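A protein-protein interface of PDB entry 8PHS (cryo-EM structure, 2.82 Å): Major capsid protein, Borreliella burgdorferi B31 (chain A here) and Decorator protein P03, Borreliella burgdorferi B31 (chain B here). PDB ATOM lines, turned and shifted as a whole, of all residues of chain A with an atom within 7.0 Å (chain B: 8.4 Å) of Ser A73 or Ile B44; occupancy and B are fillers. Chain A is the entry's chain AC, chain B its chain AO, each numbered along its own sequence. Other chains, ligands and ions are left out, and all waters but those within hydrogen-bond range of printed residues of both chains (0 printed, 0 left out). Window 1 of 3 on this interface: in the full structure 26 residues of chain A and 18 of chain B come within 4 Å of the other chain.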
ATOM      1  N   LYS A  48     -33.515  12.307 -34.330  1.00  0.00           N
ATOM      2  CA  LYS A  48     -33.078  11.159 -33.549  1.00  0.00           C
ATOM      3  C   LYS A  48     -32.436  11.645 -32.259  1.00  0.00           C
ATOM      4  O   LYS A  48     -31.762  12.677 -32.242  1.00  0.00           O
ATOM      5  CB  LYS A  48     -32.098  10.280 -34.334  1.00  0.00           C
ATOM      6  CG  LYS A  48     -31.723   8.989 -33.625  1.00  0.00           C
ATOM      7  CD  LYS A  48     -31.022   8.021 -34.560  1.00  0.00           C
ATOM      8  CE  LYS A  48     -30.757   6.691 -33.874  1.00  0.00           C
ATOM      9  NZ  LYS A  48     -30.185   5.685 -34.810  1.00  0.00           N
ATOM     10  N   TRP A  49     -32.661  10.907 -31.177  1.00  0.00           N
ATOM     11  CA  TRP A  49     -32.149  11.263 -29.863  1.00  0.00           C
ATOM     12  C   TRP A  49     -31.119  10.237 -29.413  1.00  0.00           C
ATOM     13  O   TRP A  49     -31.269   9.038 -29.671  1.00  0.00           O
ATOM     14  CB  TRP A  49     -33.284  11.351 -28.843  1.00  0.00           C
ATOM     15  CG  TRP A  49     -34.187  12.521 -29.059  1.00  0.00           C
ATOM     16  CD1 TRP A  49     -35.349  12.537 -29.772  1.00  0.00           C
ATOM     17  CD2 TRP A  49     -34.001  13.851 -28.563  1.00  0.00           C
ATOM     18  NE1 TRP A  49     -35.901  13.794 -29.749  1.00  0.00           N
ATOM     19  CE2 TRP A  49     -35.092  14.619 -29.013  1.00  0.00           C
ATOM     20  CE3 TRP A  49     -33.019  14.466 -27.783  1.00  0.00           C
ATOM     21  CZ2 TRP A  49     -35.230  15.970 -28.707  1.00  0.00           C
ATOM     22  CZ3 TRP A  49     -33.159  15.806 -27.477  1.00  0.00           C
ATOM     23  CH2 TRP A  49     -34.254  16.544 -27.940  1.00  0.00           C
ATOM     24  N   ASP A  50     -30.075  10.712 -28.739  1.00  0.00           N
ATOM     25  CA  ASP A  50     -29.005   9.849 -28.261  1.00  0.00           C
ATOM     26  C   ASP A  50     -28.617  10.268 -26.851  1.00  0.00           C
ATOM     27  O   ASP A  50     -28.805  11.419 -26.453  1.00  0.00           O
ATOM     28  CB  ASP A  50     -27.784   9.902 -29.188  1.00  0.00           C
ATOM     29  CG  ASP A  50     -26.862   8.714 -29.004  1.00  0.00           C
ATOM     30  OD1 ASP A  50     -27.084   7.925 -28.063  1.00  0.00           O
ATOM     31  OD2 ASP A  50     -25.913   8.568 -29.805  1.00  0.00           O
ATOM     32  N   ALA A  51     -28.067   9.317 -26.099  1.00  0.00           N
ATOM     33  CA  ALA A  51     -27.636   9.551 -24.730  1.00  0.00           C
ATOM     34  C   ALA A  51     -26.193   9.105 -24.564  1.00  0.00           C
ATOM     35  O   ALA A  51     -25.714   8.219 -25.276  1.00  0.00           O
ATOM     36  CB  ALA A  51     -28.527   8.813 -23.726  1.00  0.00           C
ATOM     37  N   PHE A  52     -25.501   9.731 -23.615  1.00  0.00           N
ATOM     38  CA  PHE A  52     -24.097   9.428 -23.380  1.00  0.00           C
ATOM     39  C   PHE A  52     -23.774   9.631 -21.908  1.00  0.00           C
ATOM     40  O   PHE A  52     -24.468  10.356 -21.191  1.00  0.00           O
ATOM     41  CB  PHE A  52     -23.177  10.294 -24.249  1.00  0.00           C
ATOM     42  CG  PHE A  52     -23.561  11.746 -24.286  1.00  0.00           C
ATOM     43  CD1 PHE A  52     -24.480  12.214 -25.208  1.00  0.00           C
ATOM     44  CD2 PHE A  52     -22.995  12.645 -23.397  1.00  0.00           C
ATOM     45  CE1 PHE A  52     -24.832  13.549 -25.242  1.00  0.00           C
ATOM     46  CE2 PHE A  52     -23.341  13.981 -23.427  1.00  0.00           C
ATOM     47  CZ  PHE A  52     -24.261  14.433 -24.350  1.00  0.00           C
ATOM     48  N   GLY A  71     -25.717  12.828 -20.292  1.00  0.00           N
ATOM     49  CA  GLY A  71     -26.104  13.847 -21.238  1.00  0.00           C
ATOM     50  C   GLY A  71     -26.917  13.294 -22.393  1.00  0.00           C
ATOM     51  O   GLY A  71     -26.888  12.102 -22.688  1.00  0.00           O
ATOM     52  N   PHE A  72     -27.648  14.189 -23.053  1.00  0.00           N
ATOM     53  CA  PHE A  72     -28.476  13.835 -24.194  1.00  0.00           C
ATOM     54  C   PHE A  72     -28.188  14.777 -25.353  1.00  0.00           C
ATOM     55  O   PHE A  72     -27.766  15.920 -25.158  1.00  0.00           O
ATOM     56  CB  PHE A  72     -29.968  13.890 -23.851  1.00  0.00           C
ATOM     57  CG  PHE A  72     -30.356  13.029 -22.685  1.00  0.00           C
ATOM     58  CD1 PHE A  72     -30.315  13.527 -21.394  1.00  0.00           C
ATOM     59  CD2 PHE A  72     -30.771  11.724 -22.879  1.00  0.00           C
ATOM     60  CE1 PHE A  72     -30.675  12.738 -20.321  1.00  0.00           C
ATOM     61  CE2 PHE A  72     -31.132  10.931 -21.810  1.00  0.00           C
ATOM     62  CZ  PHE A  72     -31.084  11.439 -20.529  1.00  0.00           C
ATOM     63  N   SER A  73     -28.421  14.283 -26.566  1.00  0.00           N
ATOM     64  CA  SER A  73     -28.214  15.063 -27.776  1.00  0.00           C
ATOM     65  C   SER A  73     -29.277  14.701 -28.800  1.00  0.00           C
ATOM     66  O   SER A  73     -29.848  13.608 -28.778  1.00  0.00           O
ATOM     67  CB  SER A  73     -26.814  14.836 -28.364  1.00  0.00           C
ATOM     68  OG  SER A  73     -26.658  13.500 -28.805  1.00  0.00           O
ATOM     69  N   SER A  74     -29.542  15.641 -29.704  1.00  0.00           N
ATOM     70  CA  SER A  74     -30.530  15.464 -30.761  1.00  0.00           C
ATOM     71  C   SER A  74     -29.871  15.746 -32.101  1.00  0.00           C
ATOM     72  O   SER A  74     -29.315  16.830 -32.303  1.00  0.00           O
ATOM     73  CB  SER A  74     -31.732  16.389 -30.557  1.00  0.00           C
ATOM     74  OG  SER A  74     -31.318  17.736 -30.423  1.00  0.00           O
ATOM     75  N   GLU A  75     -29.929  14.776 -33.005  1.00  0.00           N
ATOM     76  CA  GLU A  75     -29.454  14.955 -34.367  1.00  0.00           C
ATOM     77  C   GLU A  75     -30.639  15.106 -35.311  1.00  0.00           C
ATOM     78  O   GLU A  75     -31.672  14.445 -35.149  1.00  0.00           O
ATOM     79  CB  GLU A  75     -28.566  13.787 -34.803  1.00  0.00           C
ATOM     80  CG  GLU A  75     -29.276  12.451 -34.922  1.00  0.00           C
ATOM     81  CD  GLU A  75     -28.492  11.452 -35.749  1.00  0.00           C
ATOM     82  OE1 GLU A  75     -27.402  11.813 -36.240  1.00  0.00           O
ATOM     83  OE2 GLU A  75     -28.964  10.306 -35.905  1.00  0.00           O
ATOM     84  N   LYS B  23     -23.941  26.188 -30.016  1.00  0.00           N
ATOM     85  CA  LYS B  23     -23.839  24.994 -29.182  1.00  0.00           C
ATOM     86  C   LYS B  23     -24.271  23.751 -29.950  1.00  0.00           C
ATOM     87  O   LYS B  23     -23.605  22.711 -29.889  1.00  0.00           O
ATOM     88  CB  LYS B  23     -24.670  25.164 -27.910  1.00  0.00           C
ATOM     89  CG  LYS B  23     -26.061  25.731 -28.137  1.00  0.00           C
ATOM     90  CD  LYS B  23     -26.877  25.718 -26.854  1.00  0.00           C
ATOM     91  CE  LYS B  23     -26.964  24.320 -26.268  1.00  0.00           C
ATOM     92  NZ  LYS B  23     -27.881  24.273 -25.098  1.00  0.00           N
ATOM     93  N   ASN B  24     -25.378  23.839 -30.681  1.00  0.00           N
ATOM     94  CA  ASN B  24     -25.828  22.750 -31.537  1.00  0.00           C
ATOM     95  C   ASN B  24     -25.263  22.922 -32.944  1.00  0.00           C
ATOM     96  O   ASN B  24     -25.090  24.053 -33.406  1.00  0.00           O
ATOM     97  CB  ASN B  24     -27.352  22.704 -31.602  1.00  0.00           C
ATOM     98  CG  ASN B  24     -27.984  22.390 -30.261  1.00  0.00           C
ATOM     99  OD1 ASN B  24     -27.289  22.191 -29.265  1.00  0.00           O
ATOM    100  ND2 ASN B  24     -29.310  22.342 -30.230  1.00  0.00           N
ATOM    101  N   PRO B  25     -24.954  21.817 -33.635  1.00  0.00           N
ATOM    102  CA  PRO B  25     -24.437  21.924 -35.007  1.00  0.00           C
ATOM    103  C   PRO B  25     -25.375  22.703 -35.914  1.00  0.00           C
ATOM    104  O   PRO B  25     -26.547  22.343 -36.063  1.00  0.00           O
ATOM    105  CB  PRO B  25     -24.308  20.460 -35.456  1.00  0.00           C
ATOM    106  CG  PRO B  25     -25.073  19.656 -34.442  1.00  0.00           C
ATOM    107  CD  PRO B  25     -24.990  20.424 -33.167  1.00  0.00           C
ATOM    108  N   SER B  33     -27.218   8.006 -36.487  1.00  0.00           N
ATOM    109  CA  SER B  33     -26.252   7.550 -35.498  1.00  0.00           C
ATOM    110  C   SER B  33     -26.382   6.047 -35.277  1.00  0.00           C
ATOM    111  O   SER B  33     -27.468   5.471 -35.383  1.00  0.00           O
ATOM    112  CB  SER B  33     -26.446   8.295 -34.177  1.00  0.00           C
ATOM    113  OG  SER B  33     -27.692   7.971 -33.586  1.00  0.00           O
ATOM    114  N   ASP B  40     -16.638   7.189 -25.040  1.00  0.00           N
ATOM    115  CA  ASP B  40     -16.229   8.396 -25.757  1.00  0.00           C
ATOM    116  C   ASP B  40     -17.359   8.929 -26.638  1.00  0.00           C
ATOM    117  O   ASP B  40     -17.227   9.084 -27.853  1.00  0.00           O
ATOM    118  CB  ASP B  40     -14.961   8.141 -26.576  1.00  0.00           C
ATOM    119  CG  ASP B  40     -13.748   7.893 -25.704  1.00  0.00           C
ATOM    120  OD1 ASP B  40     -13.878   7.993 -24.466  1.00  0.00           O
ATOM    121  OD2 ASP B  40     -12.665   7.599 -26.253  1.00  0.00           O
ATOM    122  N   GLN B  41     -18.491   9.212 -25.993  1.00  0.00           N
ATOM    123  CA  GLN B  41     -19.650   9.783 -26.667  1.00  0.00           C
ATOM    124  C   GLN B  41     -20.040  11.144 -26.102  1.00  0.00           C
ATOM    125  O   GLN B  41     -21.050  11.714 -26.530  1.00  0.00           O
ATOM    126  CB  GLN B  41     -20.841   8.824 -26.586  1.00  0.00           C
ATOM    127  CG  GLN B  41     -20.524   7.395 -26.991  1.00  0.00           C
ATOM    128  CD  GLN B  41     -20.348   7.240 -28.488  1.00  0.00           C
ATOM    129  OE1 GLN B  41     -21.267   7.506 -29.263  1.00  0.00           O
ATOM    130  NE2 GLN B  41     -19.165   6.804 -28.902  1.00  0.00           N
ATOM    131  N   ASN B  42     -19.268  11.680 -25.158  1.00  0.00           N
ATOM    132  CA  ASN B  42     -19.582  12.946 -24.508  1.00  0.00           C
ATOM    133  C   ASN B  42     -18.680  14.086 -24.963  1.00  0.00           C
ATOM    134  O   ASN B  42     -18.691  15.155 -24.346  1.00  0.00           O
ATOM    135  CB  ASN B  42     -19.496  12.795 -22.988  1.00  0.00           C
ATOM    136  CG  ASN B  42     -18.146  12.281 -22.530  1.00  0.00           C
ATOM    137  OD1 ASN B  42     -17.321  11.866 -23.340  1.00  0.00           O
ATOM    138  ND2 ASN B  42     -17.911  12.318 -21.226  1.00  0.00           N
ATOM    139  N   LEU B  43     -17.905  13.889 -26.026  1.00  0.00           N
ATOM    140  CA  LEU B  43     -16.954  14.899 -26.475  1.00  0.00           C
ATOM    141  C   LEU B  43     -17.594  15.985 -27.327  1.00  0.00           C
ATOM    142  O   LEU B  43     -16.891  16.905 -27.758  1.00  0.00           O
ATOM    143  CB  LEU B  43     -15.814  14.243 -27.262  1.00  0.00           C
ATOM    144  CG  LEU B  43     -14.640  13.629 -26.490  1.00  0.00           C
ATOM    145  CD1 LEU B  43     -13.891  14.703 -25.719  1.00  0.00           C
ATOM    146  CD2 LEU B  43     -15.070  12.496 -25.571  1.00  0.00           C
ATOM    147  N   ILE B  44     -18.903  15.904 -27.580  1.00  0.00           N
ATOM    148  CA  ILE B  44     -19.558  16.871 -28.452  1.00  0.00           C
ATOM    149  C   ILE B  44     -19.556  18.255 -27.812  1.00  0.00           C
ATOM    150  O   ILE B  44     -19.489  18.416 -26.587  1.00  0.00           O
ATOM    151  CB  ILE B  44     -20.988  16.415 -28.784  1.00  0.00           C
ATOM    152  CG1 ILE B  44     -21.777  16.173 -27.497  1.00  0.00           C
ATOM    153  CG2 ILE B  44     -20.961  15.161 -29.643  1.00  0.00           C
ATOM    154  CD1 ILE B  44     -23.138  15.555 -27.721  1.00  0.00           C
ATOM    155  N   PHE B  45     -19.628  19.279 -28.668  1.00  0.00           N
ATOM    156  CA  PHE B  45     -19.679  20.654 -28.183  1.00  0.00           C
ATOM    157  C   PHE B  45     -21.027  20.978 -27.555  1.00  0.00           C
ATOM    158  O   PHE B  45     -21.111  21.857 -26.690  1.00  0.00           O
ATOM    159  CB  PHE B  45     -19.382  21.625 -29.325  1.00  0.00           C
ATOM    160  CG  PHE B  45     -19.104  23.029 -28.873  1.00  0.00           C
ATOM    161  CD1 PHE B  45     -18.082  23.294 -27.978  1.00  0.00           C
ATOM    162  CD2 PHE B  45     -19.860  24.086 -29.349  1.00  0.00           C
ATOM    163  CE1 PHE B  45     -17.823  24.585 -27.563  1.00  0.00           C
ATOM    164  CE2 PHE B  45     -19.605  25.380 -28.938  1.00  0.00           C
ATOM    165  CZ  PHE B  45     -18.585  25.629 -28.043  1.00  0.00           C
ATOM    166  N   SER B  46     -22.085  20.283 -27.972  1.00  0.00           N
ATOM    167  CA  SER B  46     -23.423  20.519 -27.443  1.00  0.00           C
ATOM    168  C   SER B  46     -23.607  19.988 -26.029  1.00  0.00           C
ATOM    169  O   SER B  46     -24.703  20.128 -25.476  1.00  0.00           O
ATOM    170  CB  SER B  46     -24.469  19.892 -28.369  1.00  0.00           C
ATOM    171  OG  SER B  46     -24.070  18.601 -28.789  1.00  0.00           O
ATOM    172  N   ASN B  47     -22.579  19.385 -25.434  1.00  0.00           N
ATOM    173  CA  ASN B  47     -22.674  18.881 -24.070  1.00  0.00           C
ATOM    174  C   ASN B  47     -22.649  20.042 -23.086  1.00  0.00           C
ATOM    175  O   ASN B  47     -21.590  20.391 -22.555  1.00  0.00           O
ATOM    176  CB  ASN B  47     -21.535  17.900 -23.784  1.00  0.00           C
ATOM    177  CG  ASN B  47     -21.635  17.264 -22.408  1.00  0.00           C
ATOM    178  OD1 ASN B  47     -22.594  17.490 -21.669  1.00  0.00           O
ATOM    179  ND2 ASN B  47     -20.637  16.463 -22.058  1.00  0.00           N
ATOM    180  N   SER B  48     -23.808  20.646 -22.839  1.00  0.00           N
ATOM    181  CA  SER B  48     -23.901  21.777 -21.932  1.00  0.00           C
ATOM    182  C   SER B  48     -23.921  21.303 -20.481  1.00  0.00           C
ATOM    183  O   SER B  48     -24.103  20.120 -20.184  1.00  0.00           O
ATOM    184  CB  SER B  48     -25.147  22.605 -22.240  1.00  0.00           C
ATOM    185  OG  SER B  48     -26.309  21.797 -22.216  1.00  0.00           O
ATOM    186  N   TYR B  69     -20.492  31.229 -24.753  1.00  0.00           N
ATOM    187  CA  TYR B  69     -20.762  29.837 -24.407  1.00  0.00           C
ATOM    188  C   TYR B  69     -19.480  29.084 -24.074  1.00  0.00           C
ATOM    189  O   TYR B  69     -18.491  29.161 -24.809  1.00  0.00           O
ATOM    190  CB  TYR B  69     -21.485  29.147 -25.562  1.00  0.00           C
ATOM    191  CG  TYR B  69     -21.866  27.715 -25.278  1.00  0.00           C
ATOM    192  CD1 TYR B  69     -22.734  27.402 -24.243  1.00  0.00           C
ATOM    193  CD2 TYR B  69     -21.361  26.675 -26.044  1.00  0.00           C
ATOM    194  CE1 TYR B  69     -23.088  26.096 -23.977  1.00  0.00           C
ATOM    195  CE2 TYR B  69     -21.710  25.365 -25.787  1.00  0.00           C
ATOM    196  CZ  TYR B  69     -22.573  25.083 -24.753  1.00  0.00           C
ATOM    197  OH  TYR B  69     -22.925  23.779 -24.491  1.00  0.00           O
ATOM    198  N   LYS B  70     -19.511  28.345 -22.962  1.00  0.00           N
ATOM    199  CA  LYS B  70     -18.377  27.544 -22.491  1.00  0.00           C
ATOM    200  C   LYS B  70     -17.123  28.397 -22.310  1.00  0.00           C
ATOM    201  O   LYS B  70     -16.003  27.949 -22.561  1.00  0.00           O
ATOM    202  CB  LYS B  70     -18.104  26.365 -23.426  1.00  0.00           C
ATOM    203  CG  LYS B  70     -19.025  25.176 -23.209  1.00  0.00           C
ATOM    204  CD  LYS B  70     -18.543  23.960 -23.979  1.00  0.00           C
ATOM    205  CE  LYS B  70     -19.429  22.755 -23.718  1.00  0.00           C
ATOM    206  NZ  LYS B  70     -19.392  22.343 -22.288  1.00  0.00           N
ATOM    207  N   TYR B 120     -16.397  20.715 -19.220  1.00  0.00           N
ATOM    208  CA  TYR B 120     -15.615  20.969 -20.423  1.00  0.00           C
ATOM    209  C   TYR B 120     -15.693  22.447 -20.788  1.00  0.00           C
ATOM    210  O   TYR B 120     -16.787  22.990 -20.973  1.00  0.00           O
ATOM    211  CB  TYR B 120     -16.117  20.099 -21.572  1.00  0.00           C
ATOM    212  CG  TYR B 120     -15.661  18.662 -21.482  1.00  0.00           C
ATOM    213  CD1 TYR B 120     -14.322  18.328 -21.626  1.00  0.00           C
ATOM    214  CD2 TYR B 120     -16.569  17.639 -21.240  1.00  0.00           C
ATOM    215  CE1 TYR B 120     -13.901  17.016 -21.541  1.00  0.00           C
ATOM    216  CE2 TYR B 120     -16.155  16.325 -21.152  1.00  0.00           C
ATOM    217  CZ  TYR B 120     -14.820  16.020 -21.302  1.00  0.00           C
ATOM    218  OH  TYR B 120     -14.401  14.712 -21.216  1.00  0.00           O
ATOM    219  N   HIS B 164      -9.043  18.262 -26.359  1.00  0.00           N
ATOM    220  CA  HIS B 164      -9.766  17.524 -27.382  1.00  0.00           C
ATOM    221  C   HIS B 164     -10.146  18.491 -28.492  1.00  0.00           C
ATOM    222  O   HIS B 164     -10.726  19.549 -28.226  1.00  0.00           O
ATOM    223  CB  HIS B 164     -11.018  16.857 -26.807  1.00  0.00           C
ATOM    224  CG  HIS B 164     -10.802  16.213 -25.472  1.00  0.00           C
ATOM    225  ND1 HIS B 164     -10.023  15.088 -25.305  1.00  0.00           N
ATOM    226  CD2 HIS B 164     -11.264  16.537 -24.242  1.00  0.00           C
ATOM    227  CE1 HIS B 164     -10.017  14.746 -24.030  1.00  0.00           C
ATOM    228  NE2 HIS B 164     -10.761  15.609 -23.362  1.00  0.00           N
ATOM    229  N   LEU B 166     -12.226  19.772 -31.560  1.00  0.00           N
ATOM    230  CA  LEU B 166     -13.523  19.699 -32.221  1.00  0.00           C
ATOM    231  C   LEU B 166     -13.490  20.294 -33.620  1.00  0.00           C
ATOM    232  O   LEU B 166     -14.055  19.716 -34.553  1.00  0.00           O
ATOM    233  CB  LEU B 166     -14.581  20.424 -31.384  1.00  0.00           C
ATOM    234  CG  LEU B 166     -14.744  19.942 -29.942  1.00  0.00           C
ATOM    235  CD1 LEU B 166     -15.921  20.630 -29.280  1.00  0.00           C
ATOM    236  CD2 LEU B 166     -14.911  18.433 -29.898  1.00  0.00           C
ATOM    237  N   LEU B 170     -11.013  24.987 -32.577  1.00  0.00           N
ATOM    238  CA  LEU B 170     -11.798  24.780 -31.366  1.00  0.00           C
ATOM    239  C   LEU B 170     -11.242  23.595 -30.586  1.00  0.00           C
ATOM    240  O   LEU B 170     -11.218  22.466 -31.090  1.00  0.00           O
ATOM    241  CB  LEU B 170     -13.269  24.553 -31.709  1.00  0.00           C
ATOM    242  CG  LEU B 170     -14.236  24.467 -30.529  1.00  0.00           C
ATOM    243  CD1 LEU B 170     -14.365  25.823 -29.853  1.00  0.00           C
ATOM    244  CD2 LEU B 170     -15.593  23.963 -30.987  1.00  0.00           C
ATOM    245  N   ILE B 172     -11.389  21.815 -26.519  1.00  0.00           N
ATOM    246  CA  ILE B 172     -12.068  21.798 -25.229  1.00  0.00           C
ATOM    247  C   ILE B 172     -11.270  20.939 -24.259  1.00  0.00           C
ATOM    248  O   ILE B 172     -10.627  19.959 -24.645  1.00  0.00           O
ATOM    249  CB  ILE B 172     -13.522  21.294 -25.341  1.00  0.00           C
ATOM    250  CG1 ILE B 172     -13.564  19.895 -25.956  1.00  0.00           C
ATOM    251  CG2 ILE B 172     -14.363  22.266 -26.152  1.00  0.00           C
ATOM    252  CD1 ILE B 172     -14.923  19.238 -25.876  1.00  0.00           C
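Among the printed residues, pairs that only touch across the chains: Phe A52 with Gln B41, Phe A52 with Asn B42, Phe A52 with Ile B44, Ser A73 with Ile B44 and Phe A52 with Asn B47.
Of the 10 printed residues of chain A, 4 touch a printed residue of chain B.
Printed residues of chain A that touch a printed residue of chain B: Lys A48, Phe A52, Ser A73 and Glu A75.
Hydrophobic or aromatic side chains of chain B within 4 Å of the printed part of chain A: Ile B44.
The side-chain carboxylate of Glu A75 sits at hydrogen-bond distance from the backbone NH of Ser B33 (2.9 Å).
The backbone carbonyl oxygen (O) of Ser B33 sits at hydrogen-bond distance from the side-chain amino group (NZ) of Lys A48, at 2.8 Å.
Of the printed residues of chain B, Phe A52 touches Gln B41 (3.4 Å), Asn B42 (3.5 Å), Ile B44 (3.6 Å) and Asn B47 (3.8 Å).
No residue of chain B comes within 4 Å of Ser A74.
Of the printed residues of chain A, Ser B33 touches Lys A48 (2.8 Å) and Glu A75 (2.9 Å).
Printed residues of chain A within 4 Å of Gln B41: Phe A52.
Of the printed residues of chain A, Ile B44 touches Phe A52 and Ser A73.
Of the printed residues of chain A, Asn B47 touches Phe A52.
The nearest residue of chain B that does not touch Ser A73 is Ser B46 (4.7 Å).
The nearest printed residue of chain B that does not touch Lys A48 is Pro B25 (9.9 Å).
The backbone carbonyl oxygen (O) of Lys A48 lies within hydrogen-bond range of the backbone NH (N) of Glu A75, at 2.9 Å.
O of Asp A50 lies within hydrogen-bond range of N of Ser A73, 2.9 Å away.
The side-chain amino group (NZ) of Lys B70 sits at hydrogen-bond distance from the backbone carbonyl oxygen (O) of Asn B47.
The backbone carbonyl oxygen (O) of Asn B42 lies within hydrogen-bond range of the side-chain amide nitrogen (ND2) of Asn B47 (3.3 Å).
The backbone NH of Phe A52 lies within hydrogen-bond range of the backbone carbonyl oxygen of Gly A71, 2.9 Å away.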
